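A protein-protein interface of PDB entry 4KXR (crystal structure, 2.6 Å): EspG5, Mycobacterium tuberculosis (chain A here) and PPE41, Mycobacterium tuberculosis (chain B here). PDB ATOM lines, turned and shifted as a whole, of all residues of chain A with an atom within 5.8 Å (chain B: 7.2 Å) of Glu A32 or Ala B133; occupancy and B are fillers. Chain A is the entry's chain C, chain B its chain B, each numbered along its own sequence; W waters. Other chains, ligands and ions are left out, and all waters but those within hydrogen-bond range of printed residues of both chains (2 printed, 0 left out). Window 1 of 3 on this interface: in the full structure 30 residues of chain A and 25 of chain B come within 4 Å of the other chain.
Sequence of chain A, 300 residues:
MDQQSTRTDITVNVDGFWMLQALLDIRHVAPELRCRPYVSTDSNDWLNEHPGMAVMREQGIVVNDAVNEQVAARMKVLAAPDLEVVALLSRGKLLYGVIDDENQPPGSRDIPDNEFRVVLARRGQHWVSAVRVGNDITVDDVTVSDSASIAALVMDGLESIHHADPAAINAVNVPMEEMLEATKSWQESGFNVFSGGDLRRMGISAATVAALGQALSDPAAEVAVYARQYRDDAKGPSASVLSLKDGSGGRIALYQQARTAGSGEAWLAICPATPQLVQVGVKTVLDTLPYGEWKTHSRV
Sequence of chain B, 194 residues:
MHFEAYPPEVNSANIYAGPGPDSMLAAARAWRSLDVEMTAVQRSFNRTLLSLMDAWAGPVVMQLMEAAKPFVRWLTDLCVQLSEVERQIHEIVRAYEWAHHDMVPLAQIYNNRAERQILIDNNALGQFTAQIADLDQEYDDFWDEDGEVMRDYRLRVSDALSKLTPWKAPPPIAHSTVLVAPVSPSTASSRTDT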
ATOM      1  N   VAL A  29      -8.017  31.509 -13.337  1.00  0.00           N
ATOM      2  CA  VAL A  29      -8.565  31.890 -12.025  1.00  0.00           C
ATOM      3  C   VAL A  29      -7.659  31.237 -10.983  1.00  0.00           C
ATOM      4  O   VAL A  29      -6.666  30.607 -11.345  1.00  0.00           O
ATOM      5  CB  VAL A  29     -10.035  31.448 -11.810  1.00  0.00           C
ATOM      6  CG1 VAL A  29     -10.986  32.333 -12.594  1.00  0.00           C
ATOM      7  CG2 VAL A  29     -10.226  29.990 -12.182  1.00  0.00           C
ATOM      8  N   ALA A  30      -7.997  31.381  -9.704  1.00  0.00           N
ATOM      9  CA  ALA A  30      -7.219  30.772  -8.620  1.00  0.00           C
ATOM     10  C   ALA A  30      -6.827  29.340  -8.938  1.00  0.00           C
ATOM     11  O   ALA A  30      -7.654  28.539  -9.366  1.00  0.00           O
ATOM     12  CB  ALA A  30      -7.986  30.804  -7.312  1.00  0.00           C
ATOM     13  N   PRO A  31      -5.561  29.006  -8.711  1.00  0.00           N
ATOM     14  CA  PRO A  31      -5.117  27.665  -9.015  1.00  0.00           C
ATOM     15  C   PRO A  31      -5.726  26.603  -8.123  1.00  0.00           C
ATOM     16  O   PRO A  31      -5.678  25.406  -8.464  1.00  0.00           O
ATOM     17  CB  PRO A  31      -3.605  27.737  -8.822  1.00  0.00           C
ATOM     18  CG  PRO A  31      -3.343  28.971  -8.036  1.00  0.00           C
ATOM     19  CD  PRO A  31      -4.475  29.895  -8.277  1.00  0.00           C
ATOM     20  N   GLU A  32      -6.287  27.017  -6.984  1.00  0.00           N
ATOM     21  CA  GLU A  32      -6.917  26.061  -6.058  1.00  0.00           C
ATOM     22  C   GLU A  32      -8.199  25.517  -6.611  1.00  0.00           C
ATOM     23  O   GLU A  32      -8.641  24.459  -6.193  1.00  0.00           O
ATOM     24  CB  GLU A  32      -7.196  26.684  -4.703  1.00  0.00           C
ATOM     25  CG  GLU A  32      -5.936  26.910  -3.891  1.00  0.00           C
ATOM     26  CD  GLU A  32      -5.267  28.238  -4.198  1.00  0.00           C
ATOM     27  OE1 GLU A  32      -5.760  28.981  -5.091  1.00  0.00           O
ATOM     28  OE2 GLU A  32      -4.240  28.537  -3.538  1.00  0.00           O
ATOM     29  N   LEU A  33      -8.800  26.219  -7.562  1.00  0.00           N
ATOM     30  CA  LEU A  33     -10.002  25.696  -8.216  1.00  0.00           C
ATOM     31  C   LEU A  33      -9.688  24.610  -9.244  1.00  0.00           C
ATOM     32  O   LEU A  33     -10.585  23.894  -9.657  1.00  0.00           O
ATOM     33  CB  LEU A  33     -10.805  26.834  -8.830  1.00  0.00           C
ATOM     34  CG  LEU A  33     -11.221  27.915  -7.821  1.00  0.00           C
ATOM     35  CD1 LEU A  33     -11.821  29.141  -8.511  1.00  0.00           C
ATOM     36  CD2 LEU A  33     -12.208  27.343  -6.819  1.00  0.00           C
ATOM     37  N   ARG A  34      -8.409  24.478  -9.614  1.00  0.00           N
ATOM     38  CA  ARG A  34      -7.918  23.501 -10.595  1.00  0.00           C
ATOM     39  C   ARG A  34      -8.741  23.382 -11.851  1.00  0.00           C
ATOM     40  O   ARG A  34      -9.165  22.290 -12.222  1.00  0.00           O
ATOM     41  CB  ARG A  34      -7.744  22.132  -9.971  1.00  0.00           C
ATOM     42  CG  ARG A  34      -6.354  21.934  -9.417  1.00  0.00           C
ATOM     43  CD  ARG A  34      -6.049  20.488  -9.113  1.00  0.00           C
ATOM     44  NE  ARG A  34      -4.823  20.466  -8.344  1.00  0.00           N
ATOM     45  CZ  ARG A  34      -4.318  19.392  -7.778  1.00  0.00           C
ATOM     46  NH1 ARG A  34      -4.924  18.223  -7.910  1.00  0.00           N
ATOM     47  NH2 ARG A  34      -3.196  19.484  -7.089  1.00  0.00           N
ATOM     48  N   VAL A  86      -7.739  32.036   0.793  1.00  0.00           N
ATOM     49  CA  VAL A  86      -7.953  30.629   0.488  1.00  0.00           C
ATOM     50  C   VAL A  86      -8.018  29.736   1.732  1.00  0.00           C
ATOM     51  O   VAL A  86      -7.244  29.918   2.680  1.00  0.00           O
ATOM     52  CB  VAL A  86      -6.804  30.097  -0.393  1.00  0.00           C
ATOM     53  CG1 VAL A  86      -7.036  28.625  -0.757  1.00  0.00           C
ATOM     54  CG2 VAL A  86      -6.640  30.979  -1.631  1.00  0.00           C
ATOM     55  N   LEU A  88      -7.992  25.518   2.422  1.00  0.00           N
ATOM     56  CA  LEU A  88      -8.018  24.074   2.084  1.00  0.00           C
ATOM     57  C   LEU A  88      -8.503  23.200   3.256  1.00  0.00           C
ATOM     58  O   LEU A  88      -7.804  23.082   4.255  1.00  0.00           O
ATOM     59  CB  LEU A  88      -6.642  23.579   1.663  1.00  0.00           C
ATOM     60  CG  LEU A  88      -5.880  24.420   0.644  1.00  0.00           C
ATOM     61  CD1 LEU A  88      -4.611  23.667   0.220  1.00  0.00           C
ATOM     62  CD2 LEU A  88      -6.755  24.793  -0.544  1.00  0.00           C
ATOM     63  N   ILE A 111      -9.381  16.511  -7.832  1.00  0.00           N
ATOM     64  CA  ILE A 111      -8.901  16.764  -6.475  1.00  0.00           C
ATOM     65  C   ILE A 111      -9.243  15.546  -5.608  1.00  0.00           C
ATOM     66  O   ILE A 111     -10.162  14.783  -5.918  1.00  0.00           O
ATOM     67  CB  ILE A 111      -9.473  18.061  -5.870  1.00  0.00           C
ATOM     68  CG1 ILE A 111     -10.990  18.043  -5.828  1.00  0.00           C
ATOM     69  CG2 ILE A 111      -9.034  19.280  -6.679  1.00  0.00           C
ATOM     70  CD1 ILE A 111     -11.560  19.129  -4.940  1.00  0.00           C
ATOM     71  N   ARG A 117     -12.143  22.858  -1.359  1.00  0.00           N
ATOM     72  CA  ARG A 117     -11.352  24.078  -1.535  1.00  0.00           C
ATOM     73  C   ARG A 117     -12.267  25.280  -1.607  1.00  0.00           C
ATOM     74  O   ARG A 117     -13.205  25.285  -2.387  1.00  0.00           O
ATOM     75  CB  ARG A 117     -10.570  24.018  -2.835  1.00  0.00           C
ATOM     76  CG  ARG A 117      -9.266  23.276  -2.748  1.00  0.00           C
ATOM     77  CD  ARG A 117      -9.128  22.259  -3.857  1.00  0.00           C
ATOM     78  NE  ARG A 117      -7.928  21.494  -3.595  1.00  0.00           N
ATOM     79  CZ  ARG A 117      -6.752  21.701  -4.158  1.00  0.00           C
ATOM     80  NH1 ARG A 117      -6.590  22.625  -5.107  1.00  0.00           N
ATOM     81  NH2 ARG A 117      -5.733  20.933  -3.783  1.00  0.00           N
ATOM     82  N   VAL A 119     -12.159  29.447  -2.164  1.00  0.00           N
ATOM     83  CA  VAL A 119     -11.488  30.699  -2.498  1.00  0.00           C
ATOM     84  C   VAL A 119     -12.495  31.816  -2.277  1.00  0.00           C
ATOM     85  O   VAL A 119     -13.620  31.741  -2.757  1.00  0.00           O
ATOM     86  CB  VAL A 119     -10.967  30.709  -3.960  1.00  0.00           C
ATOM     87  CG1 VAL A 119     -10.442  32.094  -4.372  1.00  0.00           C
ATOM     88  CG2 VAL A 119      -9.875  29.660  -4.141  1.00  0.00           C
ATOM     89  N   ARG A 132     -14.765  24.552  -4.517  1.00  0.00           N
ATOM     90  CA  ARG A 132     -14.645  23.322  -5.278  1.00  0.00           C
ATOM     91  C   ARG A 132     -14.712  22.083  -4.375  1.00  0.00           C
ATOM     92  O   ARG A 132     -13.957  21.970  -3.413  1.00  0.00           O
ATOM     93  CB  ARG A 132     -13.366  23.315  -6.097  1.00  0.00           C
ATOM     94  CG  ARG A 132     -13.120  21.938  -6.675  1.00  0.00           C
ATOM     95  CD  ARG A 132     -12.449  21.935  -8.021  1.00  0.00           C
ATOM     96  NE  ARG A 132     -12.447  20.579  -8.520  1.00  0.00           N
ATOM     97  CZ  ARG A 132     -11.748  20.162  -9.559  1.00  0.00           C
ATOM     98  NH1 ARG A 132     -10.983  21.008 -10.252  1.00  0.00           N
ATOM     99  NH2 ARG A 132     -11.823  18.889  -9.910  1.00  0.00           N
ATOM    100  N   TYR A 226      -4.687  30.695   3.882  1.00  0.00           N
ATOM    101  CA  TYR A 226      -3.676  31.667   3.461  1.00  0.00           C
ATOM    102  C   TYR A 226      -4.287  32.620   2.462  1.00  0.00           C
ATOM    103  O   TYR A 226      -5.469  32.504   2.150  1.00  0.00           O
ATOM    104  CB  TYR A 226      -2.450  30.962   2.899  1.00  0.00           C
ATOM    105  CG  TYR A 226      -2.767  30.048   1.750  1.00  0.00           C
ATOM    106  CD1 TYR A 226      -3.250  28.765   1.977  1.00  0.00           C
ATOM    107  CD2 TYR A 226      -2.596  30.461   0.440  1.00  0.00           C
ATOM    108  CE1 TYR A 226      -3.547  27.917   0.931  1.00  0.00           C
ATOM    109  CE2 TYR A 226      -2.897  29.622  -0.611  1.00  0.00           C
ATOM    110  CZ  TYR A 226      -3.366  28.355  -0.355  1.00  0.00           C
ATOM    111  OH  TYR A 226      -3.666  27.524  -1.381  1.00  0.00           O
ATOM    112  N   ARG A 228      -3.544  35.852  -0.890  1.00  0.00           N
ATOM    113  CA  ARG A 228      -2.767  36.427  -1.971  1.00  0.00           C
ATOM    114  C   ARG A 228      -3.290  37.830  -2.331  1.00  0.00           C
ATOM    115  O   ARG A 228      -4.495  38.070  -2.358  1.00  0.00           O
ATOM    116  CB  ARG A 228      -2.882  35.532  -3.196  1.00  0.00           C
ATOM    117  CG  ARG A 228      -1.653  34.711  -3.512  1.00  0.00           C
ATOM    118  CD  ARG A 228      -1.859  33.914  -4.797  1.00  0.00           C
ATOM    119  NE  ARG A 228      -2.457  32.610  -4.513  1.00  0.00           N
ATOM    120  CZ  ARG A 228      -3.696  32.243  -4.811  1.00  0.00           C
ATOM    121  NH1 ARG A 228      -4.525  33.061  -5.447  1.00  0.00           N
ATOM    122  NH2 ARG A 228      -4.109  31.033  -4.476  1.00  0.00           N
ATOM    123  N   LYS A 235       2.376  40.080  -7.873  1.00  0.00           N
ATOM    124  CA  LYS A 235       1.516  39.405  -6.875  1.00  0.00           C
ATOM    125  C   LYS A 235       2.361  38.968  -5.676  1.00  0.00           C
ATOM    126  O   LYS A 235       3.581  39.057  -5.715  1.00  0.00           O
ATOM    127  CB  LYS A 235       0.797  38.189  -7.478  1.00  0.00           C
ATOM    128  CG  LYS A 235       1.729  37.203  -8.179  1.00  0.00           C
ATOM    129  CD  LYS A 235       1.089  35.836  -8.400  1.00  0.00           C
ATOM    130  CE  LYS A 235       2.134  34.725  -8.524  1.00  0.00           C
ATOM    131  NZ  LYS A 235       1.600  33.380  -8.132  1.00  0.00           N
ATOM    132  N   ARG B 116       7.579  21.074  -5.764  1.00  0.00           N
ATOM    133  CA  ARG B 116       6.295  20.985  -5.102  1.00  0.00           C
ATOM    134  C   ARG B 116       6.204  19.756  -4.193  1.00  0.00           C
ATOM    135  O   ARG B 116       5.688  19.844  -3.088  1.00  0.00           O
ATOM    136  CB  ARG B 116       5.185  20.954  -6.148  1.00  0.00           C
ATOM    137  CG  ARG B 116       3.776  20.919  -5.590  1.00  0.00           C
ATOM    138  CD  ARG B 116       2.791  20.407  -6.623  1.00  0.00           C
ATOM    139  NE  ARG B 116       1.452  20.821  -6.245  1.00  0.00           N
ATOM    140  CZ  ARG B 116       0.592  20.105  -5.520  1.00  0.00           C
ATOM    141  NH1 ARG B 116       0.886  18.879  -5.109  1.00  0.00           N
ATOM    142  NH2 ARG B 116      -0.593  20.622  -5.217  1.00  0.00           N
ATOM    143  N   LEU B 119       8.153  20.328  -0.878  1.00  0.00           N
ATOM    144  CA  LEU B 119       7.430  21.183   0.052  1.00  0.00           C
ATOM    145  C   LEU B 119       6.341  20.392   0.778  1.00  0.00           C
ATOM    146  O   LEU B 119       6.153  20.560   1.988  1.00  0.00           O
ATOM    147  CB  LEU B 119       6.843  22.414  -0.639  1.00  0.00           C
ATOM    148  CG  LEU B 119       7.841  23.427  -1.218  1.00  0.00           C
ATOM    149  CD1 LEU B 119       7.094  24.685  -1.639  1.00  0.00           C
ATOM    150  CD2 LEU B 119       8.978  23.807  -0.275  1.00  0.00           C
ATOM    151  N   PHE B 128       4.225  25.864   4.293  1.00  0.00           N
ATOM    152  CA  PHE B 128       4.654  25.930   2.900  1.00  0.00           C
ATOM    153  C   PHE B 128       3.481  25.971   1.954  1.00  0.00           C
ATOM    154  O   PHE B 128       3.671  26.015   0.750  1.00  0.00           O
ATOM    155  CB  PHE B 128       5.537  24.731   2.555  1.00  0.00           C
ATOM    156  CG  PHE B 128       6.837  24.723   3.286  1.00  0.00           C
ATOM    157  CD1 PHE B 128       7.739  25.771   3.127  1.00  0.00           C
ATOM    158  CD2 PHE B 128       7.166  23.679   4.136  1.00  0.00           C
ATOM    159  CE1 PHE B 128       8.948  25.780   3.812  1.00  0.00           C
ATOM    160  CE2 PHE B 128       8.375  23.678   4.816  1.00  0.00           C
ATOM    161  CZ  PHE B 128       9.266  24.730   4.651  1.00  0.00           C
ATOM    162  N   THR B 129       2.269  25.992   2.499  1.00  0.00           N
ATOM    163  CA  THR B 129       1.059  25.795   1.698  1.00  0.00           C
ATOM    164  C   THR B 129       0.862  26.885   0.641  1.00  0.00           C
ATOM    165  O   THR B 129       0.368  26.601  -0.452  1.00  0.00           O
ATOM    166  CB  THR B 129      -0.184  25.696   2.596  1.00  0.00           C
ATOM    167  OG1 THR B 129       0.103  24.819   3.699  1.00  0.00           O
ATOM    168  CG2 THR B 129      -1.371  25.168   1.826  1.00  0.00           C
ATOM    169  N   ALA B 130       1.249  28.119   0.942  1.00  0.00           N
ATOM    170  CA  ALA B 130       1.082  29.182  -0.030  1.00  0.00           C
ATOM    171  C   ALA B 130       2.150  29.056  -1.108  1.00  0.00           C
ATOM    172  O   ALA B 130       1.909  29.386  -2.277  1.00  0.00           O
ATOM    173  CB  ALA B 130       1.148  30.541   0.640  1.00  0.00           C
ATOM    174  N   GLN B 131       3.328  28.565  -0.729  1.00  0.00           N
ATOM    175  CA  GLN B 131       4.390  28.378  -1.697  1.00  0.00           C
ATOM    176  C   GLN B 131       4.027  27.233  -2.615  1.00  0.00           C
ATOM    177  O   GLN B 131       4.271  27.304  -3.819  1.00  0.00           O
ATOM    178  CB  GLN B 131       5.717  28.103  -1.029  1.00  0.00           C
ATOM    179  CG  GLN B 131       6.242  29.243  -0.186  1.00  0.00           C
ATOM    180  CD  GLN B 131       7.545  28.867   0.483  1.00  0.00           C
ATOM    181  OE1 GLN B 131       8.258  27.986   0.015  1.00  0.00           O
ATOM    182  NE2 GLN B 131       7.858  29.518   1.581  1.00  0.00           N
ATOM    183  N   ILE B 132       3.436  26.189  -2.054  1.00  0.00           N
ATOM    184  CA  ILE B 132       2.843  25.135  -2.856  1.00  0.00           C
ATOM    185  C   ILE B 132       1.842  25.668  -3.886  1.00  0.00           C
ATOM    186  O   ILE B 132       1.884  25.245  -5.050  1.00  0.00           O
ATOM    187  CB  ILE B 132       2.179  24.055  -1.986  1.00  0.00           C
ATOM    188  CG1 ILE B 132       3.261  23.196  -1.327  1.00  0.00           C
ATOM    189  CG2 ILE B 132       1.285  23.144  -2.828  1.00  0.00           C
ATOM    190  CD1 ILE B 132       2.741  22.339  -0.194  1.00  0.00           C
ATOM    191  N   ALA B 133       0.960  26.590  -3.501  1.00  0.00           N
ATOM    192  CA  ALA B 133       0.027  27.169  -4.485  1.00  0.00           C
ATOM    193  C   ALA B 133       0.713  28.053  -5.533  1.00  0.00           C
ATOM    194  O   ALA B 133       0.249  28.103  -6.658  1.00  0.00           O
ATOM    195  CB  ALA B 133      -1.107  27.934  -3.816  1.00  0.00           C
ATOM    196  N   ASP B 134       1.778  28.765  -5.170  1.00  0.00           N
ATOM    197  CA  ASP B 134       2.535  29.567  -6.165  1.00  0.00           C
ATOM    198  C   ASP B 134       3.084  28.644  -7.245  1.00  0.00           C
ATOM    199  O   ASP B 134       3.061  28.992  -8.412  1.00  0.00           O
ATOM    200  CB  ASP B 134       3.714  30.349  -5.547  1.00  0.00           C
ATOM    201  CG  ASP B 134       3.275  31.598  -4.728  1.00  0.00           C
ATOM    202  OD1 ASP B 134       2.161  32.143  -4.937  1.00  0.00           O
ATOM    203  OD2 ASP B 134       4.081  32.044  -3.864  1.00  0.00           O
ATOM    204  N   LEU B 135       3.572  27.467  -6.845  1.00  0.00           N
ATOM    205  CA  LEU B 135       4.103  26.491  -7.788  1.00  0.00           C
ATOM    206  C   LEU B 135       2.997  25.940  -8.681  1.00  0.00           C
ATOM    207  O   LEU B 135       3.244  25.599  -9.822  1.00  0.00           O
ATOM    208  CB  LEU B 135       4.804  25.337  -7.061  1.00  0.00           C
ATOM    209  CG  LEU B 135       6.172  25.634  -6.446  1.00  0.00           C
ATOM    210  CD1 LEU B 135       6.604  24.509  -5.523  1.00  0.00           C
ATOM    211  CD2 LEU B 135       7.206  25.860  -7.526  1.00  0.00           C
ATOM    212  N   ASP B 136       1.783  25.832  -8.163  1.00  0.00           N
ATOM    213  CA  ASP B 136       0.683  25.359  -8.986  1.00  0.00           C
ATOM    214  C   ASP B 136       0.313  26.445  -9.993  1.00  0.00           C
ATOM    215  O   ASP B 136      -0.137  26.159 -11.093  1.00  0.00           O
ATOM    216  CB  ASP B 136      -0.537  24.985  -8.133  1.00  0.00           C
ATOM    217  CG  ASP B 136      -0.382  23.644  -7.426  1.00  0.00           C
ATOM    218  OD1 ASP B 136       0.537  22.858  -7.771  1.00  0.00           O
ATOM    219  OD2 ASP B 136      -1.182  23.371  -6.499  1.00  0.00           O
ATOM    220  N   GLN B 137       0.486  27.698  -9.614  1.00  0.00           N
ATOM    221  CA  GLN B 137       0.167  28.791 -10.527  1.00  0.00           C
ATOM    222  C   GLN B 137       1.198  28.804 -11.636  1.00  0.00           C
ATOM    223  O   GLN B 137       0.852  29.029 -12.781  1.00  0.00           O
ATOM    224  CB  GLN B 137       0.136  30.147  -9.803  1.00  0.00           C
ATOM    225  CG  GLN B 137      -0.230  31.315 -10.698  1.00  0.00           C
ATOM    226  CD  GLN B 137      -1.592  31.148 -11.334  1.00  0.00           C
ATOM    227  OE1 GLN B 137      -2.614  31.329 -10.672  1.00  0.00           O
ATOM    228  NE2 GLN B 137      -1.619  30.809 -12.628  1.00  0.00           N
ATOM    229  N   GLU B 138       2.460  28.566 -11.266  1.00  0.00           N
ATOM    230  CA  GLU B 138       3.570  28.480 -12.210  1.00  0.00           C
ATOM    231  C   GLU B 138       3.327  27.350 -13.194  1.00  0.00           C
ATOM    232  O   GLU B 138       3.537  27.532 -14.382  1.00  0.00           O
ATOM    233  CB  GLU B 138       4.910  28.256 -11.489  1.00  0.00           C
ATOM    234  CG  GLU B 138       6.106  28.706 -12.310  1.00  0.00           C
ATOM    235  CD  GLU B 138       7.466  28.154 -11.875  1.00  0.00           C
ATOM    236  OE1 GLU B 138       7.574  27.184 -11.085  1.00  0.00           O
ATOM    237  OE2 GLU B 138       8.468  28.709 -12.381  1.00  0.00           O
ATOM    238  N   TYR B 139       2.890  26.189 -12.711  1.00  0.00           N
ATOM    239  CA  TYR B 139       2.600  25.054 -13.608  1.00  0.00           C
ATOM    240  C   TYR B 139       1.492  25.440 -14.604  1.00  0.00           C
ATOM    241  O   TYR B 139       1.608  25.210 -15.813  1.00  0.00           O
ATOM    242  CB  TYR B 139       2.240  23.806 -12.788  1.00  0.00           C
ATOM    243  CG  TYR B 139       1.881  22.571 -13.591  1.00  0.00           C
ATOM    244  CD1 TYR B 139       2.861  21.740 -14.105  1.00  0.00           C
ATOM    245  CD2 TYR B 139       0.556  22.233 -13.813  1.00  0.00           C
ATOM    246  CE1 TYR B 139       2.529  20.621 -14.855  1.00  0.00           C
ATOM    247  CE2 TYR B 139       0.216  21.130 -14.555  1.00  0.00           C
ATOM    248  CZ  TYR B 139       1.199  20.326 -15.068  1.00  0.00           C
ATOM    249  OH  TYR B 139       0.839  19.227 -15.777  1.00  0.00           O
ATOM    250  N   ASP B 140       0.441  26.063 -14.089  1.00  0.00           N
ATOM    251  CA  ASP B 140      -0.647  26.556 -14.929  1.00  0.00           C
ATOM    252  C   ASP B 140      -0.173  27.586 -15.973  1.00  0.00           C
ATOM    253  O   ASP B 140      -0.729  27.672 -17.083  1.00  0.00           O
ATOM    254  CB  ASP B 140      -1.758  27.153 -14.064  1.00  0.00           C
ATOM    255  CG  ASP B 140      -2.653  26.090 -13.414  1.00  0.00           C
ATOM    256  OD1 ASP B 140      -2.583  24.894 -13.792  1.00  0.00           O
ATOM    257  OD2 ASP B 140      -3.444  26.453 -12.510  1.00  0.00           O
HETATM  258  O   HOH W   1      -3.954  22.901  -7.305  1.00  0.00           O
HETATM  259  O   HOH W   2       3.427  31.366  -9.496  1.00  0.00           O
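NZ of Lys A235 lies within salt-bridge range of OD1 of Asp B134 (3.5 Å). The guanidinium group (NH2) of Arg B116 lies close to the guanidinium group (NH2) of Arg A34 (3.4 Å).
Water W2 lies within hydrogen-bond range of the backbone carbonyl oxygen (O) of Asp B134 (2.6 Å), the side-chain amino group (NZ) of Lys A235 (3.0 Å) and the backbone NH (N) of Glu B138 (3.5 Å). Water W1 lies within hydrogen-bond range of the guanidinium group (NE) of Arg A34 (2.8 Å), the side-chain carboxylate (OD2) of Asp B136 (2.9 Å), the backbone carbonyl oxygen (O) of Pro A31 (3.3 Å) and the guanidinium group (NH1) of Arg A117 (3.4 Å).
Of the printed residues of chain B, Tyr A226 touches Thr B129 (3.6 Å), Ala B130 (3.8 Å) and Ala B133 (3.6 Å). Of the printed residues of chain A, Arg B116 touches Arg A34 (3.4 Å). Of the printed residues of chain A, Thr B129 touches Leu A88 and Tyr A226. Of the printed residues of chain A, Asp B134 touches Lys A235. The nearest residue of chain B that does not touch Glu A32 is Thr B129 (5.9 Å). The nearest printed residue of chain A that does not touch Asp B140 is Val A29 (5.4 Å).
Pro A31 touches Ala B133 (CG to O, 3.9 Å). Pro A31 touches Gln B137. Asp B140 touches Pro A31 (OD2 to CB, 3.9 Å). Glu A32 touches Ala B133 (OE2 to CB, 3.2 Å). Leu A88 touches Thr B129 (CD1 to CG2, 3.9 Å). Tyr A226 touches Thr B129. Tyr A226 touches Ala B130. Tyr A226 touches Ala B133 (OH to CB, 3.6 Å). Gln B137 touches Lys A235.
Of the 15 printed residues of chain A, 6 touch a printed residue of chain B. Printed residues of chain A that touch a printed residue of chain B: Pro A31, Glu A32, Arg A34, Leu A88, Tyr A226 and Lys A235. Hydrophobic or aromatic side chains of chain A within 4 Å of the printed part of chain B: Pro A31, Leu A88 and Tyr A226. Along chain A the printed residues that touch a printed residue of chain B span positions 31 to 235. Of the 15 printed residues of chain B, 7 touch a printed residue of chain A. Hydrophobic or aromatic side chains of chain B that line the printed part of chain A: Ala B130 and Ala B133.
OE2 of Glu A32 sits at hydrogen-bond distance from OH of Tyr A226 (2.5 Å). The backbone carbonyl oxygen (O) of Glu A32 lies within hydrogen-bond range of the guanidinium group (NH1) of Arg A117, 3.0 Å away. The backbone carbonyl oxygen (O) of Tyr A226 sits at hydrogen-bond distance from the backbone NH (N) of Val A86. The backbone carbonyl oxygen (O) of Arg A34 sits at hydrogen-bond distance from the guanidinium group (NH1) of Arg A132, 3.0 Å away. NE of Arg B116 is in salt-bridge range of OD1 of Asp B136. The guanidinium group (NH2) of Arg A228 lies within salt-bridge range of the side-chain carboxylate (OE2) of Glu A32.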
